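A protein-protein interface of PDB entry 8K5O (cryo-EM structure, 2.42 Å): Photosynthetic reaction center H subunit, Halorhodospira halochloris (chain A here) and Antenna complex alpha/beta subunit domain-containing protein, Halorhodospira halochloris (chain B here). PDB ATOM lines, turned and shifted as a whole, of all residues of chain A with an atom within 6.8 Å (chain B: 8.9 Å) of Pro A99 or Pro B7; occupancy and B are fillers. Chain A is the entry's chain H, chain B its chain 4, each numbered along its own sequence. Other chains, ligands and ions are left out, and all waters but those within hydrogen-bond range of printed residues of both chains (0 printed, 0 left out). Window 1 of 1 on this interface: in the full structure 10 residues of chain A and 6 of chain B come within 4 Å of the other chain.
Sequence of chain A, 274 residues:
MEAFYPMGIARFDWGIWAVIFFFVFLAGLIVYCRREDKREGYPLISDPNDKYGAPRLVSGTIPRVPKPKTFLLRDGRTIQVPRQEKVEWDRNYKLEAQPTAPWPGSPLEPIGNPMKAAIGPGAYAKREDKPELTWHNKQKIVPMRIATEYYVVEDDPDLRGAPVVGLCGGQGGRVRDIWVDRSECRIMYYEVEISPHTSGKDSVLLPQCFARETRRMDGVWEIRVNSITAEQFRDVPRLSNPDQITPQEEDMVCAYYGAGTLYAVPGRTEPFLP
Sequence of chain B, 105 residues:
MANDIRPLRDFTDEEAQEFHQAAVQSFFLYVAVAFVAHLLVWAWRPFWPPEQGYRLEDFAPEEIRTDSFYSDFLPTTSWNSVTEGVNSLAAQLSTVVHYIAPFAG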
ATOM      1  N   ASP A  47      16.038   4.110 -10.048  1.00  0.00           N
ATOM      2  CA  ASP A  47      15.534   2.825 -10.508  1.00  0.00           C
ATOM      3  C   ASP A  47      15.233   2.898 -11.999  1.00  0.00           C
ATOM      4  O   ASP A  47      14.417   3.731 -12.416  1.00  0.00           O
ATOM      5  CB  ASP A  47      14.278   2.432  -9.733  1.00  0.00           C
ATOM      6  CG  ASP A  47      13.956   0.952  -9.839  1.00  0.00           C
ATOM      7  OD1 ASP A  47      14.209   0.353 -10.902  1.00  0.00           O
ATOM      8  OD2 ASP A  47      13.439   0.383  -8.855  1.00  0.00           O
ATOM      9  N   PRO A  48      15.862   2.063 -12.830  1.00  0.00           N
ATOM     10  CA  PRO A  48      15.501   2.045 -14.254  1.00  0.00           C
ATOM     11  C   PRO A  48      14.047   1.700 -14.492  1.00  0.00           C
ATOM     12  O   PRO A  48      13.458   2.170 -15.473  1.00  0.00           O
ATOM     13  CB  PRO A  48      16.438   0.980 -14.837  1.00  0.00           C
ATOM     14  CG  PRO A  48      17.575   0.919 -13.892  1.00  0.00           C
ATOM     15  CD  PRO A  48      17.010   1.193 -12.538  1.00  0.00           C
ATOM     16  N   ASN A  49      13.448   0.892 -13.622  1.00  0.00           N
ATOM     17  CA  ASN A  49      12.028   0.603 -13.723  1.00  0.00           C
ATOM     18  C   ASN A  49      11.243   1.844 -13.328  1.00  0.00           C
ATOM     19  O   ASN A  49      10.965   2.069 -12.148  1.00  0.00           O
ATOM     20  CB  ASN A  49      11.655  -0.584 -12.843  1.00  0.00           C
ATOM     21  CG  ASN A  49      10.210  -0.975 -12.985  1.00  0.00           C
ATOM     22  OD1 ASN A  49       9.672  -1.000 -14.088  1.00  0.00           O
ATOM     23  ND2 ASN A  49       9.571  -1.284 -11.870  1.00  0.00           N
ATOM     24  N   LEU A  95      20.492  -9.481 -15.427  1.00  0.00           N
ATOM     25  CA  LEU A  95      19.499  -9.560 -14.366  1.00  0.00           C
ATOM     26  C   LEU A  95      18.850 -10.935 -14.284  1.00  0.00           C
ATOM     27  O   LEU A  95      18.781 -11.523 -13.200  1.00  0.00           O
ATOM     28  CB  LEU A  95      18.427  -8.491 -14.571  1.00  0.00           C
ATOM     29  CG  LEU A  95      18.875  -7.043 -14.420  1.00  0.00           C
ATOM     30  CD1 LEU A  95      17.761  -6.131 -14.885  1.00  0.00           C
ATOM     31  CD2 LEU A  95      19.255  -6.746 -12.978  1.00  0.00           C
ATOM     32  N   ALA A  97      15.803 -11.264 -14.541  1.00  0.00           N
ATOM     33  CA  ALA A  97      14.684 -10.909 -13.686  1.00  0.00           C
ATOM     34  C   ALA A  97      13.947  -9.731 -14.299  1.00  0.00           C
ATOM     35  O   ALA A  97      14.513  -8.963 -15.080  1.00  0.00           O
ATOM     36  CB  ALA A  97      15.148 -10.555 -12.269  1.00  0.00           C
ATOM     37  N   GLN A  98      12.676  -9.600 -13.934  1.00  0.00           N
ATOM     38  CA  GLN A  98      11.865  -8.470 -14.341  1.00  0.00           C
ATOM     39  C   GLN A  98      11.226  -7.822 -13.123  1.00  0.00           C
ATOM     40  O   GLN A  98      10.922  -8.512 -12.147  1.00  0.00           O
ATOM     41  CB  GLN A  98      10.762  -8.891 -15.322  1.00  0.00           C
ATOM     42  CG  GLN A  98      11.221  -9.803 -16.431  1.00  0.00           C
ATOM     43  CD  GLN A  98      10.128 -10.089 -17.442  1.00  0.00           C
ATOM     44  OE1 GLN A  98       8.949  -9.857 -17.182  1.00  0.00           O
ATOM     45  NE2 GLN A  98      10.517 -10.608 -18.601  1.00  0.00           N
ATOM     46  N   PRO A  99      11.015  -6.511 -13.143  1.00  0.00           N
ATOM     47  CA  PRO A  99      10.294  -5.876 -12.037  1.00  0.00           C
ATOM     48  C   PRO A  99       8.875  -6.415 -11.951  1.00  0.00           C
ATOM     49  O   PRO A  99       8.243  -6.711 -12.964  1.00  0.00           O
ATOM     50  CB  PRO A  99      10.318  -4.390 -12.404  1.00  0.00           C
ATOM     51  CG  PRO A  99      11.388  -4.252 -13.434  1.00  0.00           C
ATOM     52  CD  PRO A  99      11.415  -5.540 -14.172  1.00  0.00           C
ATOM     53  N   THR A 100       8.381  -6.561 -10.724  1.00  0.00           N
ATOM     54  CA  THR A 100       7.014  -7.033 -10.554  1.00  0.00           C
ATOM     55  C   THR A 100       6.006  -5.984 -10.999  1.00  0.00           C
ATOM     56  O   THR A 100       4.931  -6.330 -11.499  1.00  0.00           O
ATOM     57  CB  THR A 100       6.767  -7.428  -9.101  1.00  0.00           C
ATOM     58  OG1 THR A 100       6.944  -6.285  -8.256  1.00  0.00           O
ATOM     59  CG2 THR A 100       7.736  -8.516  -8.680  1.00  0.00           C
ATOM     60  N   ALA A 101       6.337  -4.714 -10.833  1.00  0.00           N
ATOM     61  CA  ALA A 101       5.484  -3.583 -11.151  1.00  0.00           C
ATOM     62  C   ALA A 101       6.294  -2.552 -11.920  1.00  0.00           C
ATOM     63  O   ALA A 101       7.528  -2.561 -11.868  1.00  0.00           O
ATOM     64  CB  ALA A 101       4.909  -2.959  -9.873  1.00  0.00           C
ATOM     65  N   PRO A 102       5.633  -1.660 -12.659  1.00  0.00           N
ATOM     66  CA  PRO A 102       6.354  -0.659 -13.454  1.00  0.00           C
ATOM     67  C   PRO A 102       6.827   0.566 -12.684  1.00  0.00           C
ATOM     68  O   PRO A 102       7.163   1.570 -13.316  1.00  0.00           O
ATOM     69  CB  PRO A 102       5.312  -0.261 -14.509  1.00  0.00           C
ATOM     70  CG  PRO A 102       4.017  -0.510 -13.859  1.00  0.00           C
ATOM     71  CD  PRO A 102       4.207  -1.723 -13.022  1.00  0.00           C
ATOM     72  N   TRP A 103       6.869   0.533 -11.358  1.00  0.00           N
ATOM     73  CA  TRP A 103       7.276   1.720 -10.624  1.00  0.00           C
ATOM     74  C   TRP A 103       8.603   1.494  -9.911  1.00  0.00           C
ATOM     75  O   TRP A 103       8.965   0.355  -9.607  1.00  0.00           O
ATOM     76  CB  TRP A 103       6.219   2.127  -9.590  1.00  0.00           C
ATOM     77  CG  TRP A 103       4.922   2.462 -10.209  1.00  0.00           C
ATOM     78  CD1 TRP A 103       4.540   3.665 -10.712  1.00  0.00           C
ATOM     79  CD2 TRP A 103       3.830   1.571 -10.422  1.00  0.00           C
ATOM     80  NE1 TRP A 103       3.271   3.584 -11.217  1.00  0.00           N
ATOM     81  CE2 TRP A 103       2.812   2.305 -11.049  1.00  0.00           C
ATOM     82  CE3 TRP A 103       3.612   0.224 -10.139  1.00  0.00           C
ATOM     83  CZ2 TRP A 103       1.601   1.736 -11.402  1.00  0.00           C
ATOM     84  CZ3 TRP A 103       2.407  -0.336 -10.483  1.00  0.00           C
ATOM     85  CH2 TRP A 103       1.415   0.418 -11.103  1.00  0.00           C
ATOM     86  N   SER A 106       9.983  -1.341  -7.086  1.00  0.00           N
ATOM     87  CA  SER A 106       9.388  -2.644  -7.315  1.00  0.00           C
ATOM     88  C   SER A 106      10.454  -3.728  -7.193  1.00  0.00           C
ATOM     89  O   SER A 106      11.576  -3.557  -7.681  1.00  0.00           O
ATOM     90  CB  SER A 106       8.747  -2.704  -8.695  1.00  0.00           C
ATOM     91  OG  SER A 106       7.736  -1.724  -8.822  1.00  0.00           O
ATOM     92  N   PRO A 107      10.142  -4.845  -6.550  1.00  0.00           N
ATOM     93  CA  PRO A 107      11.097  -5.952  -6.495  1.00  0.00           C
ATOM     94  C   PRO A 107      11.228  -6.630  -7.849  1.00  0.00           C
ATOM     95  O   PRO A 107      10.393  -6.474  -8.742  1.00  0.00           O
ATOM     96  CB  PRO A 107      10.482  -6.891  -5.457  1.00  0.00           C
ATOM     97  CG  PRO A 107       9.032  -6.622  -5.542  1.00  0.00           C
ATOM     98  CD  PRO A 107       8.896  -5.157  -5.832  1.00  0.00           C
ATOM     99  N   LEU A 108      12.306  -7.389  -7.995  1.00  0.00           N
ATOM    100  CA  LEU A 108      12.590  -8.120  -9.222  1.00  0.00           C
ATOM    101  C   LEU A 108      12.267  -9.590  -9.006  1.00  0.00           C
ATOM    102  O   LEU A 108      12.832 -10.230  -8.115  1.00  0.00           O
ATOM    103  CB  LEU A 108      14.050  -7.953  -9.638  1.00  0.00           C
ATOM    104  CG  LEU A 108      14.543  -6.547  -9.978  1.00  0.00           C
ATOM    105  CD1 LEU A 108      16.054  -6.502  -9.895  1.00  0.00           C
ATOM    106  CD2 LEU A 108      14.075  -6.121 -11.353  1.00  0.00           C
ATOM    107  N   GLU A 109      11.353 -10.118  -9.809  1.00  0.00           N
ATOM    108  CA  GLU A 109      11.113 -11.548  -9.841  1.00  0.00           C
ATOM    109  C   GLU A 109      11.979 -12.165 -10.929  1.00  0.00           C
ATOM    110  O   GLU A 109      11.919 -11.711 -12.080  1.00  0.00           O
ATOM    111  CB  GLU A 109       9.647 -11.847 -10.098  1.00  0.00           C
ATOM    112  CG  GLU A 109       9.384 -13.224 -10.675  1.00  0.00           C
ATOM    113  CD  GLU A 109       9.294 -14.305  -9.612  1.00  0.00           C
ATOM    114  OE1 GLU A 109       9.613 -14.021  -8.440  1.00  0.00           O
ATOM    115  OE2 GLU A 109       8.907 -15.442  -9.949  1.00  0.00           O
ATOM    116  N   ILE B   5      13.927  -5.505 -16.746  1.00  0.00           N
ATOM    117  CA  ILE B   5      13.748  -4.408 -17.689  1.00  0.00           C
ATOM    118  C   ILE B   5      12.263  -4.112 -17.861  1.00  0.00           C
ATOM    119  O   ILE B   5      11.748  -3.136 -17.315  1.00  0.00           O
ATOM    120  CB  ILE B   5      14.407  -4.727 -19.040  1.00  0.00           C
ATOM    121  CG1 ILE B   5      15.850  -5.186 -18.826  1.00  0.00           C
ATOM    122  CG2 ILE B   5      14.378  -3.509 -19.943  1.00  0.00           C
ATOM    123  CD1 ILE B   5      16.488  -5.799 -20.053  1.00  0.00           C
ATOM    124  N   ARG B   6      11.582  -4.961 -18.621  1.00  0.00           N
ATOM    125  CA  ARG B   6      10.141  -4.845 -18.791  1.00  0.00           C
ATOM    126  C   ARG B   6       9.441  -5.420 -17.568  1.00  0.00           C
ATOM    127  O   ARG B   6       9.642  -6.598 -17.252  1.00  0.00           O
ATOM    128  CB  ARG B   6       9.699  -5.586 -20.047  1.00  0.00           C
ATOM    129  CG  ARG B   6       8.214  -5.500 -20.369  1.00  0.00           C
ATOM    130  CD  ARG B   6       7.844  -4.179 -21.034  1.00  0.00           C
ATOM    131  NE  ARG B   6       7.488  -3.148 -20.068  1.00  0.00           N
ATOM    132  CZ  ARG B   6       7.276  -1.875 -20.373  1.00  0.00           C
ATOM    133  NH1 ARG B   6       7.365  -1.439 -21.619  1.00  0.00           N
ATOM    134  NH2 ARG B   6       6.970  -1.017 -19.404  1.00  0.00           N
ATOM    135  N   PRO B   7       8.635  -4.641 -16.851  1.00  0.00           N
ATOM    136  CA  PRO B   7       7.940  -5.186 -15.681  1.00  0.00           C
ATOM    137  C   PRO B   7       6.971  -6.293 -16.060  1.00  0.00           C
ATOM    138  O   PRO B   7       6.400  -6.304 -17.152  1.00  0.00           O
ATOM    139  CB  PRO B   7       7.203  -3.970 -15.106  1.00  0.00           C
ATOM    140  CG  PRO B   7       7.138  -2.995 -16.226  1.00  0.00           C
ATOM    141  CD  PRO B   7       8.394  -3.200 -17.004  1.00  0.00           C
ATOM    142  N   LEU B   8       6.804  -7.242 -15.136  1.00  0.00           N
ATOM    143  CA  LEU B   8       5.882  -8.353 -15.356  1.00  0.00           C
ATOM    144  C   LEU B   8       4.477  -7.842 -15.632  1.00  0.00           C
ATOM    145  O   LEU B   8       3.930  -8.035 -16.724  1.00  0.00           O
ATOM    146  CB  LEU B   8       5.884  -9.283 -14.143  1.00  0.00           C
ATOM    147  CG  LEU B   8       7.122 -10.148 -13.925  1.00  0.00           C
ATOM    148  CD1 LEU B   8       7.188 -10.610 -12.485  1.00  0.00           C
ATOM    149  CD2 LEU B   8       7.103 -11.332 -14.867  1.00  0.00           C
ATOM    150  N   ARG B   9       3.877  -7.187 -14.649  1.00  0.00           N
ATOM    151  CA  ARG B   9       2.622  -6.484 -14.846  1.00  0.00           C
ATOM    152  C   ARG B   9       2.901  -5.051 -15.267  1.00  0.00           C
ATOM    153  O   ARG B   9       3.756  -4.370 -14.697  1.00  0.00           O
ATOM    154  CB  ARG B   9       1.782  -6.499 -13.569  1.00  0.00           C
ATOM    155  CG  ARG B   9       0.444  -5.797 -13.703  1.00  0.00           C
ATOM    156  CD  ARG B   9      -0.394  -5.951 -12.447  1.00  0.00           C
ATOM    157  NE  ARG B   9      -0.870  -7.318 -12.274  1.00  0.00           N
ATOM    158  CZ  ARG B   9      -1.470  -7.767 -11.181  1.00  0.00           C
ATOM    159  NH1 ARG B   9      -1.664  -6.990 -10.129  1.00  0.00           N
ATOM    160  NH2 ARG B   9      -1.885  -9.031 -11.142  1.00  0.00           N
ATOM    161  N   ASP B  10       2.179  -4.601 -16.284  1.00  0.00           N
ATOM    162  CA  ASP B  10       2.278  -3.234 -16.762  1.00  0.00           C
ATOM    163  C   ASP B  10       1.016  -2.478 -16.380  1.00  0.00           C
ATOM    164  O   ASP B  10      -0.062  -3.063 -16.242  1.00  0.00           O
ATOM    165  CB  ASP B  10       2.487  -3.179 -18.275  1.00  0.00           C
ATOM    166  CG  ASP B  10       3.271  -1.958 -18.706  1.00  0.00           C
ATOM    167  OD1 ASP B  10       2.948  -0.848 -18.234  1.00  0.00           O
ATOM    168  OD2 ASP B  10       4.211  -2.107 -19.513  1.00  0.00           O
ATOM    169  N   PHE B  11       1.164  -1.173 -16.198  1.00  0.00           N
ATOM    170  CA  PHE B  11       0.079  -0.309 -15.752  1.00  0.00           C
ATOM    171  C   PHE B  11      -0.088   0.775 -16.810  1.00  0.00           C
ATOM    172  O   PHE B  11       0.603   1.796 -16.780  1.00  0.00           O
ATOM    173  CB  PHE B  11       0.398   0.265 -14.379  1.00  0.00           C
ATOM    174  CG  PHE B  11      -0.786   0.838 -13.664  1.00  0.00           C
ATOM    175  CD1 PHE B  11      -1.755   0.007 -13.136  1.00  0.00           C
ATOM    176  CD2 PHE B  11      -0.909   2.200 -13.479  1.00  0.00           C
ATOM    177  CE1 PHE B  11      -2.836   0.526 -12.462  1.00  0.00           C
ATOM    178  CE2 PHE B  11      -1.978   2.718 -12.797  1.00  0.00           C
ATOM    179  CZ  PHE B  11      -2.948   1.882 -12.295  1.00  0.00           C
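Of the 7 printed residues of chain B, 6 touch a printed residue of chain A.
Printed residues of chain B that touch a printed residue of chain A: Ile B5, Arg B6, Pro B7, Leu B8, Arg B9 and Phe B11.
Printed residues of chain A that touch a printed residue of chain B: Asn A49, Ala A97, Gln A98, Pro A99, Thr A100, Ala A101, Pro A102, Trp A103 and Glu A109.
Among the printed residues, no Asp or Glu carboxylate lies within 4 Å of a Lys or Arg side-chain nitrogen of the other chain.
Of the printed residues of chain B, Gln A98 touches Arg B6 and Leu B8.
Of chain B, only Ile B5, Arg B6, Pro B7 and Leu B8 come within 4 Å of Pro A99.
Pro B7 touches four residues of chain A.
Of the printed residues of chain A, Leu B8 touches Gln A98, Pro A99 and Glu A109.
Printed residues of chain A within 4 Å of Arg B9: Thr A100 (3.4 Å) and Pro A102 (3.2 Å).
Printed residues of chain A within 4 Å of Phe B11: Pro A102 (3.7 Å) and Trp A103 (3.3 Å).
The nearest residue of chain B that does not touch Pro A99 is Arg B9 (4.7 Å).
The nearest residue of chain A that does not touch Pro B7 is Gln A98 (4.2 Å).
The nearest printed residue of chain B that does not touch Ala A97 is Arg B6 (5.8 Å).
The backbone NH (N) of Asn A49 is in hydrogen-bond range of the side-chain carboxylate (OD1) of Asp A47.
The side-chain amide nitrogen (ND2) of Asn A49 lies within hydrogen-bond range of the backbone carbonyl oxygen (O) of Ala A101, at 2.4 Å.
O of Gln A98 lies within hydrogen-bond range of N of Glu A109 (2.9 Å).
The backbone NH (N) of Thr A100 lies within hydrogen-bond range of the backbone carbonyl oxygen (O) of Pro A107 (2.8 Å).
The backbone carbonyl oxygen (O) of Trp A103 lies within hydrogen-bond range of the side-chain hydroxyl (OG) of Ser A106 (2.5 Å).
NH2 of Arg B6 lies within salt-bridge range of OD2 of Asp B10, 3.0 Å away.
The side-chain amide oxygen of Gln A98 sits close to the backbone carbonyl oxygen of Arg B6 (3.3 Å).
O of Pro A99 lies within hydrogen-bond range of N of Leu B8 (2.7 Å).
O of Thr A100 sits at hydrogen-bond distance from N of Arg B9 (3.4 Å).
Asn A49 touches Pro B7.
O of Ala A97 touches N of Ile B5, 3.9 Å away.
OE1 of Gln A98 touches CD2 of Leu B8 (3.3 Å).
N of Ile B5 touches CD of Pro A99, at 3.6 Å.
Arg B6 touches Pro A99 (O to CD, 3.7 Å).
Pro A99 touches Pro B7.
Pro B7 touches Pro A102 (CG to CA, 3.7 Å).
Phe B11 touches Pro A102 (CB to CG, 3.7 Å).
CZ2 of Trp A103 touches CD2 of Phe B11, at 3.3 Å.
Leu B8 touches Glu A109 (CD1 to CB, 3.6 Å).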
